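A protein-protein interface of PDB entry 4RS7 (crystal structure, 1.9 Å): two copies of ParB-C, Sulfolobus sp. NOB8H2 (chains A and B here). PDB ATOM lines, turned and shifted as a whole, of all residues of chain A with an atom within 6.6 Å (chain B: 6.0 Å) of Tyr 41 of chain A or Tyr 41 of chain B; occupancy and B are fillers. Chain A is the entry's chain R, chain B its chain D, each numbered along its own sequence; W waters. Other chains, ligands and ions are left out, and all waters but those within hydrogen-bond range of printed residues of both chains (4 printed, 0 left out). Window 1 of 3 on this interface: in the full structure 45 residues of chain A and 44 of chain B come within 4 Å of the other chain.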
ATOM      1  N   ASN A  36       1.540   9.212 -24.437  1.00  0.00           N
ATOM      2  CA  ASN A  36       0.339   8.847 -23.692  1.00  0.00           C
ATOM      3  C   ASN A  36       0.363   9.361 -22.255  1.00  0.00           C
ATOM      4  O   ASN A  36      -0.669   9.755 -21.702  1.00  0.00           O
ATOM      5  CB  ASN A  36       0.128   7.329 -23.700  1.00  0.00           C
ATOM      6  CG  ASN A  36      -0.227   6.790 -25.079  1.00  0.00           C
ATOM      7  OD1 ASN A  36      -0.528   7.551 -26.002  1.00  0.00           O
ATOM      8  ND2 ASN A  36      -0.205   5.470 -25.219  1.00  0.00           N
ATOM      9  N   MET A  37       1.549   9.354 -21.659  1.00  0.00           N
ATOM     10  CA  MET A  37       1.730   9.796 -20.281  1.00  0.00           C
ATOM     11  C   MET A  37       1.299  11.251 -20.091  1.00  0.00           C
ATOM     12  O   MET A  37       0.775  11.623 -19.034  1.00  0.00           O
ATOM     13  CB  MET A  37       3.194   9.638 -19.877  1.00  0.00           C
ATOM     14  CG  MET A  37       3.415   9.514 -18.396  1.00  0.00           C
ATOM     15  SD  MET A  37       3.004   7.721 -17.774  1.00  0.00           S
ATOM     16  CE  MET A  37       4.778   6.921 -17.890  1.00  0.00           C
ATOM     17  N   GLU A  38       1.528  12.076 -21.106  1.00  0.00           N
ATOM     18  CA  GLU A  38       1.165  13.487 -21.012  1.00  0.00           C
ATOM     19  C   GLU A  38      -0.330  13.655 -20.746  1.00  0.00           C
ATOM     20  O   GLU A  38      -0.736  14.506 -19.953  1.00  0.00           O
ATOM     21  CB  GLU A  38       1.573  14.252 -22.277  1.00  0.00           C
ATOM     22  CG  GLU A  38       1.355  15.760 -22.180  1.00  0.00           C
ATOM     23  CD  GLU A  38       1.887  16.524 -23.390  1.00  0.00           C
ATOM     24  OE1 GLU A  38       2.238  15.890 -24.404  1.00  0.00           O
ATOM     25  OE2 GLU A  38       1.960  17.766 -23.324  1.00  0.00           O
ATOM     26  N   ALA A  39      -1.144  12.833 -21.400  1.00  0.00           N
ATOM     27  CA  ALA A  39      -2.594  12.929 -21.262  1.00  0.00           C
ATOM     28  C   ALA A  39      -3.054  12.714 -19.819  1.00  0.00           C
ATOM     29  O   ALA A  39      -4.042  13.298 -19.380  1.00  0.00           O
ATOM     30  CB  ALA A  39      -3.288  11.955 -22.202  1.00  0.00           C
ATOM     31  N   ILE A  40      -2.330  11.885 -19.075  1.00  0.00           N
ATOM     32  CA  ILE A  40      -2.689  11.632 -17.686  1.00  0.00           C
ATOM     33  C   ILE A  40      -2.537  12.905 -16.854  1.00  0.00           C
ATOM     34  O   ILE A  40      -3.418  13.260 -16.071  1.00  0.00           O
ATOM     35  CB  ILE A  40      -1.862  10.469 -17.084  1.00  0.00           C
ATOM     36  CG1 ILE A  40      -2.148   9.176 -17.850  1.00  0.00           C
ATOM     37  CG2 ILE A  40      -2.182  10.284 -15.611  1.00  0.00           C
ATOM     38  CD1 ILE A  40      -1.323   7.994 -17.408  1.00  0.00           C
ATOM     39  N   TYR A  41      -1.428  13.606 -17.039  1.00  0.00           N
ATOM     40  CA  TYR A  41      -1.192  14.830 -16.285  1.00  0.00           C
ATOM     41  C   TYR A  41      -2.108  15.969 -16.739  1.00  0.00           C
ATOM     42  O   TYR A  41      -2.470  16.841 -15.945  1.00  0.00           O
ATOM     43  CB  TYR A  41       0.297  15.194 -16.321  1.00  0.00           C
ATOM     44  CG  TYR A  41       1.114  14.155 -15.592  1.00  0.00           C
ATOM     45  CD1 TYR A  41       1.580  13.024 -16.253  1.00  0.00           C
ATOM     46  CD2 TYR A  41       1.375  14.272 -14.232  1.00  0.00           C
ATOM     47  CE1 TYR A  41       2.309  12.053 -15.587  1.00  0.00           C
ATOM     48  CE2 TYR A  41       2.105  13.299 -13.553  1.00  0.00           C
ATOM     49  CZ  TYR A  41       2.568  12.194 -14.242  1.00  0.00           C
ATOM     50  OH  TYR A  41       3.292  11.221 -13.590  1.00  0.00           O
ATOM     51  N   LYS A  42      -2.504  15.938 -18.010  1.00  0.00           N
ATOM     52  CA  LYS A  42      -3.504  16.873 -18.522  1.00  0.00           C
ATOM     53  C   LYS A  42      -4.867  16.632 -17.878  1.00  0.00           C
ATOM     54  O   LYS A  42      -5.570  17.578 -17.537  1.00  0.00           O
ATOM     55  CB  LYS A  42      -3.637  16.759 -20.044  1.00  0.00           C
ATOM     56  CG  LYS A  42      -2.576  17.512 -20.827  1.00  0.00           C
ATOM     57  CD  LYS A  42      -2.892  17.477 -22.323  1.00  0.00           C
ATOM     58  CE  LYS A  42      -2.030  18.457 -23.087  1.00  0.00           C
ATOM     59  NZ  LYS A  42      -0.596  18.243 -22.772  1.00  0.00           N
ATOM     60  N   GLN A  43      -5.236  15.360 -17.728  1.00  0.00           N
ATOM     61  CA  GLN A  43      -6.528  14.993 -17.137  1.00  0.00           C
ATOM     62  C   GLN A  43      -6.684  15.556 -15.731  1.00  0.00           C
ATOM     63  O   GLN A  43      -7.767  15.999 -15.337  1.00  0.00           O
ATOM     64  CB  GLN A  43      -6.699  13.469 -17.117  1.00  0.00           C
ATOM     65  CG  GLN A  43      -6.959  12.879 -18.493  1.00  0.00           C
ATOM     66  CD  GLN A  43      -6.592  11.410 -18.595  1.00  0.00           C
ATOM     67  OE1 GLN A  43      -6.469  10.707 -17.588  1.00  0.00           O
ATOM     68  NE2 GLN A  43      -6.409  10.937 -19.824  1.00  0.00           N
ATOM     69  N   ALA A  44      -5.591  15.534 -14.978  1.00  0.00           N
ATOM     70  CA  ALA A  44      -5.563  16.110 -13.643  1.00  0.00           C
ATOM     71  C   ALA A  44      -5.765  17.623 -13.693  1.00  0.00           C
ATOM     72  O   ALA A  44      -6.518  18.179 -12.895  1.00  0.00           O
ATOM     73  CB  ALA A  44      -4.254  15.764 -12.950  1.00  0.00           C
ATOM     74  N   SER A  45      -5.091  18.294 -14.625  1.00  0.00           N
ATOM     75  CA  SER A  45      -5.263  19.734 -14.775  1.00  0.00           C
ATOM     76  C   SER A  45      -6.710  20.056 -15.134  1.00  0.00           C
ATOM     77  O   SER A  45      -7.277  21.027 -14.638  1.00  0.00           O
ATOM     78  CB  SER A  45      -4.325  20.293 -15.853  1.00  0.00           C
ATOM     79  OG  SER A  45      -2.970  20.193 -15.460  1.00  0.00           O
ATOM     80  N   LEU A  46      -7.299  19.242 -16.008  1.00  0.00           N
ATOM     81  CA  LEU A  46      -8.694  19.425 -16.403  1.00  0.00           C
ATOM     82  C   LEU A  46      -9.663  19.320 -15.218  1.00  0.00           C
ATOM     83  O   LEU A  46     -10.592  20.122 -15.098  1.00  0.00           O
ATOM     84  CB  LEU A  46      -9.083  18.442 -17.517  1.00  0.00           C
ATOM     85  CG  LEU A  46      -8.571  18.772 -18.921  1.00  0.00           C
ATOM     86  CD1 LEU A  46      -8.637  17.551 -19.839  1.00  0.00           C
ATOM     87  CD2 LEU A  46      -9.349  19.942 -19.522  1.00  0.00           C
ATOM     88  N   PHE A  70      -3.181  24.497  -5.978  1.00  0.00           N
ATOM     89  CA  PHE A  70      -3.054  23.302  -6.815  1.00  0.00           C
ATOM     90  C   PHE A  70      -1.798  22.512  -6.466  1.00  0.00           C
ATOM     91  O   PHE A  70      -1.856  21.303  -6.249  1.00  0.00           O
ATOM     92  CB  PHE A  70      -3.040  23.668  -8.304  1.00  0.00           C
ATOM     93  CG  PHE A  70      -2.685  22.515  -9.218  1.00  0.00           C
ATOM     94  CD1 PHE A  70      -3.643  21.587  -9.591  1.00  0.00           C
ATOM     95  CD2 PHE A  70      -1.396  22.370  -9.713  1.00  0.00           C
ATOM     96  CE1 PHE A  70      -3.326  20.534 -10.434  1.00  0.00           C
ATOM     97  CE2 PHE A  70      -1.073  21.318 -10.558  1.00  0.00           C
ATOM     98  CZ  PHE A  70      -2.039  20.402 -10.918  1.00  0.00           C
ATOM     99  N   VAL A  74      -1.294  18.617  -5.079  1.00  0.00           N
ATOM    100  CA  VAL A  74      -0.836  17.506  -5.918  1.00  0.00           C
ATOM    101  C   VAL A  74       0.657  17.175  -5.856  1.00  0.00           C
ATOM    102  O   VAL A  74       1.074  16.136  -6.357  1.00  0.00           O
ATOM    103  CB  VAL A  74      -1.254  17.699  -7.396  1.00  0.00           C
ATOM    104  CG1 VAL A  74      -2.762  17.930  -7.489  1.00  0.00           C
ATOM    105  CG2 VAL A  74      -0.481  18.857  -8.032  1.00  0.00           C
ATOM    106  N   TYR A  77       1.804  13.779  -5.190  1.00  0.00           N
ATOM    107  CA  TYR A  77       1.449  12.811  -6.226  1.00  0.00           C
ATOM    108  C   TYR A  77       2.450  12.779  -7.381  1.00  0.00           C
ATOM    109  O   TYR A  77       2.392  11.890  -8.230  1.00  0.00           O
ATOM    110  CB  TYR A  77       0.060  13.120  -6.787  1.00  0.00           C
ATOM    111  CG  TYR A  77      -1.054  13.102  -5.760  1.00  0.00           C
ATOM    112  CD1 TYR A  77      -2.125  13.980  -5.864  1.00  0.00           C
ATOM    113  CD2 TYR A  77      -1.047  12.201  -4.703  1.00  0.00           C
ATOM    114  CE1 TYR A  77      -3.151  13.973  -4.942  1.00  0.00           C
ATOM    115  CE2 TYR A  77      -2.077  12.184  -3.772  1.00  0.00           C
ATOM    116  CZ  TYR A  77      -3.126  13.075  -3.901  1.00  0.00           C
ATOM    117  OH  TYR A  77      -4.157  13.079  -2.990  1.00  0.00           O
ATOM    118  N   PHE A  78       3.343  13.763  -7.421  1.00  0.00           N
ATOM    119  CA  PHE A  78       4.337  13.868  -8.490  1.00  0.00           C
ATOM    120  C   PHE A  78       5.494  12.912  -8.221  1.00  0.00           C
ATOM    121  O   PHE A  78       6.607  13.338  -7.912  1.00  0.00           O
ATOM    122  CB  PHE A  78       4.875  15.300  -8.596  1.00  0.00           C
ATOM    123  CG  PHE A  78       3.899  16.290  -9.182  1.00  0.00           C
ATOM    124  CD1 PHE A  78       4.088  17.651  -8.999  1.00  0.00           C
ATOM    125  CD2 PHE A  78       2.813  15.868  -9.928  1.00  0.00           C
ATOM    126  CE1 PHE A  78       3.207  18.573  -9.543  1.00  0.00           C
ATOM    127  CE2 PHE A  78       1.929  16.783 -10.474  1.00  0.00           C
ATOM    128  CZ  PHE A  78       2.125  18.134 -10.282  1.00  0.00           C
ATOM    129  N   ARG A  79       5.221  11.617  -8.329  1.00  0.00           N
ATOM    130  CA  ARG A  79       6.214  10.600  -8.023  1.00  0.00           C
ATOM    131  C   ARG A  79       5.816   9.285  -8.668  1.00  0.00           C
ATOM    132  O   ARG A  79       4.712   9.151  -9.192  1.00  0.00           O
ATOM    133  CB  ARG A  79       6.319  10.415  -6.505  1.00  0.00           C
ATOM    134  CG  ARG A  79       5.047   9.859  -5.868  1.00  0.00           C
ATOM    135  CD  ARG A  79       5.089   9.903  -4.336  1.00  0.00           C
ATOM    136  NE  ARG A  79       3.784   9.575  -3.766  1.00  0.00           N
ATOM    137  CZ  ARG A  79       3.354   8.338  -3.538  1.00  0.00           C
ATOM    138  NH1 ARG A  79       4.128   7.298  -3.815  1.00  0.00           N
ATOM    139  NH2 ARG A  79       2.150   8.137  -3.025  1.00  0.00           N
ATOM    140  N   PHE A  81       4.488   5.907  -7.926  1.00  0.00           N
ATOM    141  CA  PHE A  81       3.844   5.124  -6.872  1.00  0.00           C
ATOM    142  C   PHE A  81       4.482   3.741  -6.850  1.00  0.00           C
ATOM    143  O   PHE A  81       4.795   3.188  -7.900  1.00  0.00           O
ATOM    144  CB  PHE A  81       2.341   4.991  -7.129  1.00  0.00           C
ATOM    145  CG  PHE A  81       1.567   6.269  -6.935  1.00  0.00           C
ATOM    146  CD1 PHE A  81       1.820   7.379  -7.723  1.00  0.00           C
ATOM    147  CD2 PHE A  81       0.565   6.348  -5.978  1.00  0.00           C
ATOM    148  CE1 PHE A  81       1.103   8.551  -7.550  1.00  0.00           C
ATOM    149  CE2 PHE A  81      -0.157   7.516  -5.802  1.00  0.00           C
ATOM    150  CZ  PHE A  81       0.111   8.619  -6.588  1.00  0.00           C
ATOM    151  N   ASN B  36      -9.573  12.280  -5.496  1.00  0.00           N
ATOM    152  CA  ASN B  36      -9.740  11.959  -6.909  1.00  0.00           C
ATOM    153  C   ASN B  36      -8.433  12.165  -7.677  1.00  0.00           C
ATOM    154  O   ASN B  36      -8.076  11.369  -8.547  1.00  0.00           O
ATOM    155  CB  ASN B  36     -10.849  12.834  -7.502  1.00  0.00           C
ATOM    156  CG  ASN B  36     -11.517  12.207  -8.710  1.00  0.00           C
ATOM    157  OD1 ASN B  36     -10.941  11.357  -9.397  1.00  0.00           O
ATOM    158  ND2 ASN B  36     -12.746  12.635  -8.983  1.00  0.00           N
ATOM    159  N   MET B  37      -7.715  13.234  -7.349  1.00  0.00           N
ATOM    160  CA  MET B  37      -6.432  13.512  -7.991  1.00  0.00           C
ATOM    161  C   MET B  37      -5.466  12.347  -7.827  1.00  0.00           C
ATOM    162  O   MET B  37      -4.737  12.014  -8.755  1.00  0.00           O
ATOM    163  CB  MET B  37      -5.799  14.789  -7.433  1.00  0.00           C
ATOM    164  CG  MET B  37      -6.513  16.062  -7.847  1.00  0.00           C
ATOM    165  SD  MET B  37      -6.320  16.455  -9.761  1.00  0.00           S
ATOM    166  CE  MET B  37      -7.463  18.022  -9.832  1.00  0.00           C
ATOM    167  N   GLU B  38      -5.456  11.727  -6.649  1.00  0.00           N
ATOM    168  CA  GLU B  38      -4.558  10.593  -6.428  1.00  0.00           C
ATOM    169  C   GLU B  38      -4.832   9.494  -7.453  1.00  0.00           C
ATOM    170  O   GLU B  38      -3.905   8.905  -8.013  1.00  0.00           O
ATOM    171  CB  GLU B  38      -4.686  10.036  -5.005  1.00  0.00           C
ATOM    172  CG  GLU B  38      -3.758   8.863  -4.752  1.00  0.00           C
ATOM    173  CD  GLU B  38      -3.715   8.423  -3.305  1.00  0.00           C
ATOM    174  OE1 GLU B  38      -4.471   8.977  -2.479  1.00  0.00           O
ATOM    175  OE2 GLU B  38      -2.914   7.517  -2.996  1.00  0.00           O
ATOM    176  N   ALA B  39      -6.112   9.239  -7.706  1.00  0.00           N
ATOM    177  CA  ALA B  39      -6.520   8.173  -8.615  1.00  0.00           C
ATOM    178  C   ALA B  39      -6.048   8.437 -10.040  1.00  0.00           C
ATOM    179  O   ALA B  39      -5.623   7.519 -10.741  1.00  0.00           O
ATOM    180  CB  ALA B  39      -8.032   7.994  -8.578  1.00  0.00           C
ATOM    181  N   ILE B  40      -6.122   9.695 -10.464  1.00  0.00           N
ATOM    182  CA  ILE B  40      -5.672  10.072 -11.803  1.00  0.00           C
ATOM    183  C   ILE B  40      -4.166   9.877 -11.958  1.00  0.00           C
ATOM    184  O   ILE B  40      -3.714   9.206 -12.886  1.00  0.00           O
ATOM    185  CB  ILE B  40      -6.062  11.527 -12.148  1.00  0.00           C
ATOM    186  CG1 ILE B  40      -7.590  11.653 -12.211  1.00  0.00           C
ATOM    187  CG2 ILE B  40      -5.403  11.975 -13.466  1.00  0.00           C
ATOM    188  CD1 ILE B  40      -8.097  13.077 -12.338  1.00  0.00           C
ATOM    189  N   TYR B  41      -3.393  10.452 -11.042  1.00  0.00           N
ATOM    190  CA  TYR B  41      -1.933  10.376 -11.120  1.00  0.00           C
ATOM    191  C   TYR B  41      -1.415   8.948 -10.994  1.00  0.00           C
ATOM    192  O   TYR B  41      -0.365   8.607 -11.545  1.00  0.00           O
ATOM    193  CB  TYR B  41      -1.277  11.266 -10.057  1.00  0.00           C
ATOM    194  CG  TYR B  41      -1.391  12.752 -10.333  1.00  0.00           C
ATOM    195  CD1 TYR B  41      -2.157  13.575  -9.518  1.00  0.00           C
ATOM    196  CD2 TYR B  41      -0.732  13.329 -11.412  1.00  0.00           C
ATOM    197  CE1 TYR B  41      -2.260  14.937  -9.766  1.00  0.00           C
ATOM    198  CE2 TYR B  41      -0.831  14.687 -11.671  1.00  0.00           C
ATOM    199  CZ  TYR B  41      -1.593  15.486 -10.844  1.00  0.00           C
ATOM    200  OH  TYR B  41      -1.692  16.837 -11.096  1.00  0.00           O
ATOM    201  N   LYS B  42      -2.148   8.113 -10.266  1.00  0.00           N
ATOM    202  CA  LYS B  42      -1.775   6.710 -10.125  1.00  0.00           C
ATOM    203  C   LYS B  42      -1.771   5.991 -11.477  1.00  0.00           C
ATOM    204  O   LYS B  42      -1.035   5.022 -11.668  1.00  0.00           O
ATOM    205  CB  LYS B  42      -2.701   6.003  -9.126  1.00  0.00           C
ATOM    206  CG  LYS B  42      -2.012   4.929  -8.297  1.00  0.00           C
ATOM    207  CD  LYS B  42      -2.857   4.497  -7.095  1.00  0.00           C
ATOM    208  CE  LYS B  42      -4.050   3.650  -7.514  1.00  0.00           C
ATOM    209  NZ  LYS B  42      -4.776   3.082  -6.336  1.00  0.00           N
ATOM    210  N   GLN B  43      -2.583   6.472 -12.417  1.00  0.00           N
ATOM    211  CA  GLN B  43      -2.568   5.947 -13.785  1.00  0.00           C
ATOM    212  C   GLN B  43      -1.158   5.919 -14.369  1.00  0.00           C
ATOM    213  O   GLN B  43      -0.764   4.947 -15.012  1.00  0.00           O
ATOM    214  CB  GLN B  43      -3.453   6.782 -14.712  1.00  0.00           C
ATOM    215  CG  GLN B  43      -4.946   6.644 -14.507  1.00  0.00           C
ATOM    216  CD  GLN B  43      -5.727   7.274 -15.650  1.00  0.00           C
ATOM    217  OE1 GLN B  43      -6.487   6.600 -16.344  1.00  0.00           O
ATOM    218  NE2 GLN B  43      -5.533   8.572 -15.857  1.00  0.00           N
ATOM    219  N   ALA B  44      -0.406   6.996 -14.161  1.00  0.00           N
ATOM    220  CA  ALA B  44       0.940   7.089 -14.716  1.00  0.00           C
ATOM    221  C   ALA B  44       1.820   5.926 -14.265  1.00  0.00           C
ATOM    222  O   ALA B  44       2.556   5.346 -15.068  1.00  0.00           O
ATOM    223  CB  ALA B  44       1.575   8.423 -14.353  1.00  0.00           C
ATOM    224  N   SER B  45       1.738   5.581 -12.983  1.00  0.00           N
ATOM    225  CA  SER B  45       2.537   4.486 -12.442  1.00  0.00           C
ATOM    226  C   SER B  45       2.050   3.132 -12.954  1.00  0.00           C
ATOM    227  O   SER B  45       2.851   2.278 -13.328  1.00  0.00           O
ATOM    228  CB  SER B  45       2.540   4.515 -10.910  1.00  0.00           C
ATOM    229  OG  SER B  45       3.255   5.640 -10.430  1.00  0.00           O
ATOM    230  N   LEU B  46       0.736   2.938 -12.975  1.00  0.00           N
ATOM    231  CA  LEU B  46       0.164   1.706 -13.510  1.00  0.00           C
ATOM    232  C   LEU B  46       0.619   1.467 -14.956  1.00  0.00           C
ATOM    233  O   LEU B  46       1.034   0.363 -15.308  1.00  0.00           O
ATOM    234  CB  LEU B  46      -1.367   1.734 -13.413  1.00  0.00           C
ATOM    235  CG  LEU B  46      -2.160   0.439 -13.615  1.00  0.00           C
ATOM    236  CD1 LEU B  46      -3.620   0.651 -13.239  1.00  0.00           C
ATOM    237  CD2 LEU B  46      -2.055  -0.055 -15.046  1.00  0.00           C
ATOM    238  N   PHE B  70      11.888   6.870 -15.519  1.00  0.00           N
ATOM    239  CA  PHE B  70      10.513   7.327 -15.315  1.00  0.00           C
ATOM    240  C   PHE B  70      10.462   8.827 -15.037  1.00  0.00           C
ATOM    241  O   PHE B  70       9.698   9.562 -15.668  1.00  0.00           O
ATOM    242  CB  PHE B  70       9.839   6.566 -14.164  1.00  0.00           C
ATOM    243  CG  PHE B  70       8.474   7.102 -13.799  1.00  0.00           C
ATOM    244  CD1 PHE B  70       7.358   6.759 -14.544  1.00  0.00           C
ATOM    245  CD2 PHE B  70       8.313   7.951 -12.716  1.00  0.00           C
ATOM    246  CE1 PHE B  70       6.100   7.250 -14.210  1.00  0.00           C
ATOM    247  CE2 PHE B  70       7.057   8.446 -12.376  1.00  0.00           C
ATOM    248  CZ  PHE B  70       5.954   8.094 -13.127  1.00  0.00           C
ATOM    249  N   VAL B  74       8.587  11.894 -17.141  1.00  0.00           N
ATOM    250  CA  VAL B  74       7.396  12.601 -16.674  1.00  0.00           C
ATOM    251  C   VAL B  74       7.643  13.917 -15.937  1.00  0.00           C
ATOM    252  O   VAL B  74       6.697  14.662 -15.692  1.00  0.00           O
ATOM    253  CB  VAL B  74       6.489  11.688 -15.811  1.00  0.00           C
ATOM    254  CG1 VAL B  74       6.088  10.455 -16.608  1.00  0.00           C
ATOM    255  CG2 VAL B  74       7.186  11.297 -14.507  1.00  0.00           C
ATOM    256  N   TYR B  77       6.008  16.946 -16.982  1.00  0.00           N
ATOM    257  CA  TYR B  77       4.553  16.888 -16.851  1.00  0.00           C
ATOM    258  C   TYR B  77       4.095  17.256 -15.436  1.00  0.00           C
ATOM    259  O   TYR B  77       2.893  17.365 -15.179  1.00  0.00           O
ATOM    260  CB  TYR B  77       4.034  15.482 -17.178  1.00  0.00           C
ATOM    261  CG  TYR B  77       4.359  14.964 -18.570  1.00  0.00           C
ATOM    262  CD1 TYR B  77       4.503  13.601 -18.796  1.00  0.00           C
ATOM    263  CD2 TYR B  77       4.497  15.825 -19.656  1.00  0.00           C
ATOM    264  CE1 TYR B  77       4.782  13.105 -20.048  1.00  0.00           C
ATOM    265  CE2 TYR B  77       4.785  15.331 -20.928  1.00  0.00           C
ATOM    266  CZ  TYR B  77       4.924  13.966 -21.111  1.00  0.00           C
ATOM    267  OH  TYR B  77       5.208  13.443 -22.351  1.00  0.00           O
ATOM    268  N   PHE B  78       5.051  17.422 -14.525  1.00  0.00           N
ATOM    269  CA  PHE B  78       4.755  17.702 -13.121  1.00  0.00           C
ATOM    270  C   PHE B  78       4.329  19.151 -12.916  1.00  0.00           C
ATOM    271  O   PHE B  78       5.022  19.916 -12.249  1.00  0.00           O
ATOM    272  CB  PHE B  78       5.982  17.421 -12.247  1.00  0.00           C
ATOM    273  CG  PHE B  78       6.244  15.960 -11.991  1.00  0.00           C
ATOM    274  CD1 PHE B  78       7.393  15.566 -11.326  1.00  0.00           C
ATOM    275  CD2 PHE B  78       5.347  14.985 -12.401  1.00  0.00           C
ATOM    276  CE1 PHE B  78       7.648  14.230 -11.076  1.00  0.00           C
ATOM    277  CE2 PHE B  78       5.597  13.643 -12.152  1.00  0.00           C
ATOM    278  CZ  PHE B  78       6.748  13.266 -11.489  1.00  0.00           C
ATOM    279  N   ARG B  79       3.192  19.533 -13.482  1.00  0.00           N
ATOM    280  CA  ARG B  79       2.787  20.933 -13.455  1.00  0.00           C
ATOM    281  C   ARG B  79       1.302  21.072 -13.732  1.00  0.00           C
ATOM    282  O   ARG B  79       0.644  20.110 -14.120  1.00  0.00           O
ATOM    283  CB  ARG B  79       3.572  21.723 -14.503  1.00  0.00           C
ATOM    284  CG  ARG B  79       3.360  21.234 -15.927  1.00  0.00           C
ATOM    285  CD  ARG B  79       4.369  21.867 -16.902  1.00  0.00           C
ATOM    286  NE  ARG B  79       4.244  21.297 -18.240  1.00  0.00           N
ATOM    287  CZ  ARG B  79       3.386  21.731 -19.158  1.00  0.00           C
ATOM    288  NH1 ARG B  79       3.333  21.153 -20.350  1.00  0.00           N
ATOM    289  NH2 ARG B  79       2.584  22.748 -18.886  1.00  0.00           N
ATOM    290  N   PHE B  81      -0.976  22.217 -16.295  1.00  0.00           N
ATOM    291  CA  PHE B  81      -1.003  22.605 -17.700  1.00  0.00           C
ATOM    292  C   PHE B  81      -1.907  23.816 -17.849  1.00  0.00           C
ATOM    293  O   PHE B  81      -2.895  23.944 -17.126  1.00  0.00           O
ATOM    294  CB  PHE B  81      -1.503  21.453 -18.572  1.00  0.00           C
ATOM    295  CG  PHE B  81      -0.515  20.328 -18.715  1.00  0.00           C
ATOM    296  CD1 PHE B  81      -0.121  19.589 -17.610  1.00  0.00           C
ATOM    297  CD2 PHE B  81       0.019  20.009 -19.955  1.00  0.00           C
ATOM    298  CE1 PHE B  81       0.789  18.554 -17.732  1.00  0.00           C
ATOM    299  CE2 PHE B  81       0.930  18.970 -20.091  1.00  0.00           C
ATOM    300  CZ  PHE B  81       1.315  18.240 -18.975  1.00  0.00           C
HETATM  301  O   HOH W   1       4.709  14.593 -24.797  1.00  0.00           O
HETATM  302  O   HOH W   2      -0.905  17.683 -13.764  1.00  0.00           O
HETATM  303  O   HOH W   3      -5.204  11.134  -1.199  1.00  0.00           O
HETATM  304  O   HOH W   4       2.175   8.212 -10.935  1.00  0.00           O
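The side-chain amide nitrogen (NE2) of Gln 43 of chain B is in hydrogen-bond range of the side-chain amide oxygen (OE1) of Gln 43 of chain A (2.9 Å). The side-chain hydroxyl (OG) of Ser 45 of chain A lies within hydrogen-bond range of the backbone NH (N) of Phe 81 of chain B, 3.0 Å away. The backbone NH (N) of Phe 81 of chain A lies within hydrogen-bond range of the side-chain hydroxyl (OG) of Ser 45 of chain B, at 2.8 Å. The side-chain sulfur (SD) of Met 37 of chain A sits close to the backbone carbonyl oxygen (O) of Ala 44 of chain B. The backbone carbonyl oxygen of Ala 44 of chain A lies close to the side-chain sulfur of Met 37 of chain B, at 3.6 Å.
The side-chain carboxylate (OE2) of Glu 38 of chain A lies within salt-bridge range of the side-chain amino group (NZ) of Lys 42 of chain A (2.7 Å). The backbone carbonyl oxygen of Ala 39 of chain A lies close to the side-chain amide nitrogen of Gln 43 of chain A (3.4 Å). The backbone carbonyl oxygen (O) of Tyr 41 of chain A sits at hydrogen-bond distance from the side-chain hydroxyl (OG) of Ser 45 of chain A, at 3.4 Å.
Tyr 41 of chain B touches Tyr 41 of chain A (CE2 to CD2, 3.4 Å). Ala 44 of chain A touches Tyr 41 of chain B (CB to OH, 3.3 Å). Arg 79 of chain B touches Ser 45 of chain A (O to OG, 3.9 Å). Phe 78 of chain A touches Tyr 41 of chain B (CE2 to CE2, 3.7 Å). CE2 of Phe 70 of chain B touches C of Arg 79 of chain A, at 3.999 Å. N of Arg 79 of chain A touches CZ of Phe 78 of chain B, at 3.9 Å. CE2 of Phe 81 of chain A touches OE2 of Glu 38 of chain B (3.9 Å).
Of chain B, only Tyr 41 (3.4 Å), Ala 44 (3.4 Å), Val 74 (3.9 Å), Tyr 77 (3.6 Å), Phe 78 (3.6 Å) and Phe 81 (3.7 Å) come within 4 Å of Tyr 41 of chain A. Of chain A, only Tyr 41 (3.4 Å), Ala 44 (3.3 Å), Phe 70 (3.6 Å), Val 74 (3.8 Å), Tyr 77 (3.5 Å) and Phe 78 (3.7 Å) come within 4 Å of Tyr 41 of chain B. Of the printed residues of chain A, Lys 42 of chain B touches Phe 81 (3.7 Å). Of the printed residues of chain B, Gln 43 of chain A touches Gln 43 (2.9 Å). Of the printed residues of chain A, Phe 70 of chain B touches Met 37 (3.9 Å) and Arg 79 (3.999 Å). Printed residues of chain A within 4 Å of Arg 79 of chain B: Ser 45 (3.9 Å), Phe 70 (3.97 Å) and Phe 78 (3.7 Å). The nearest residue of chain A that does not touch Tyr 41 of chain B is Phe 81 of chain A (4.3 Å).
Of the 17 printed residues of chain A, 14 touch a printed residue of chain B. Hydrophobic or aromatic side chains of chain A within 4 Å of the printed part of chain B: Met 37, Ile 40, Tyr 41, Ala 44, Phe 70, Val 74, Tyr 77, Phe 78 and Phe 81. Among the printed residues, no Asp or Glu carboxylate lies within 4 Å of a Lys or Arg side-chain nitrogen of the other chain.
Glu 38 of chain A touches Tyr 77 of chain B, and with the chains exchanged Tyr 77 of chain A touches Glu 38 of chain B. Phe 70 of chain A touches Arg 79 of chain B, and with the chains exchanged Arg 79 of chain A touches Phe 70 of chain B. Positions printed for both chains: 36, 37, 38, 39, 40, 41, 42, 43, 44, 45, 46, 70, 74, 77, 78, 79 and 81.
Water W1 bridges the side-chain hydroxyl (OH) of Tyr 77 of chain B (2.7 Å) and the side-chain carboxylate (OE1) of Glu 38 of chain A (2.8 Å). Water W2 lies within hydrogen-bond range of the backbone carbonyl oxygen of Tyr 41 of chain A (2.8 Å), the backbone carbonyl oxygen of Arg 79 of chain B (2.9 Å) and the side-chain hydroxyl of Tyr 41 of chain B (2.9 Å).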
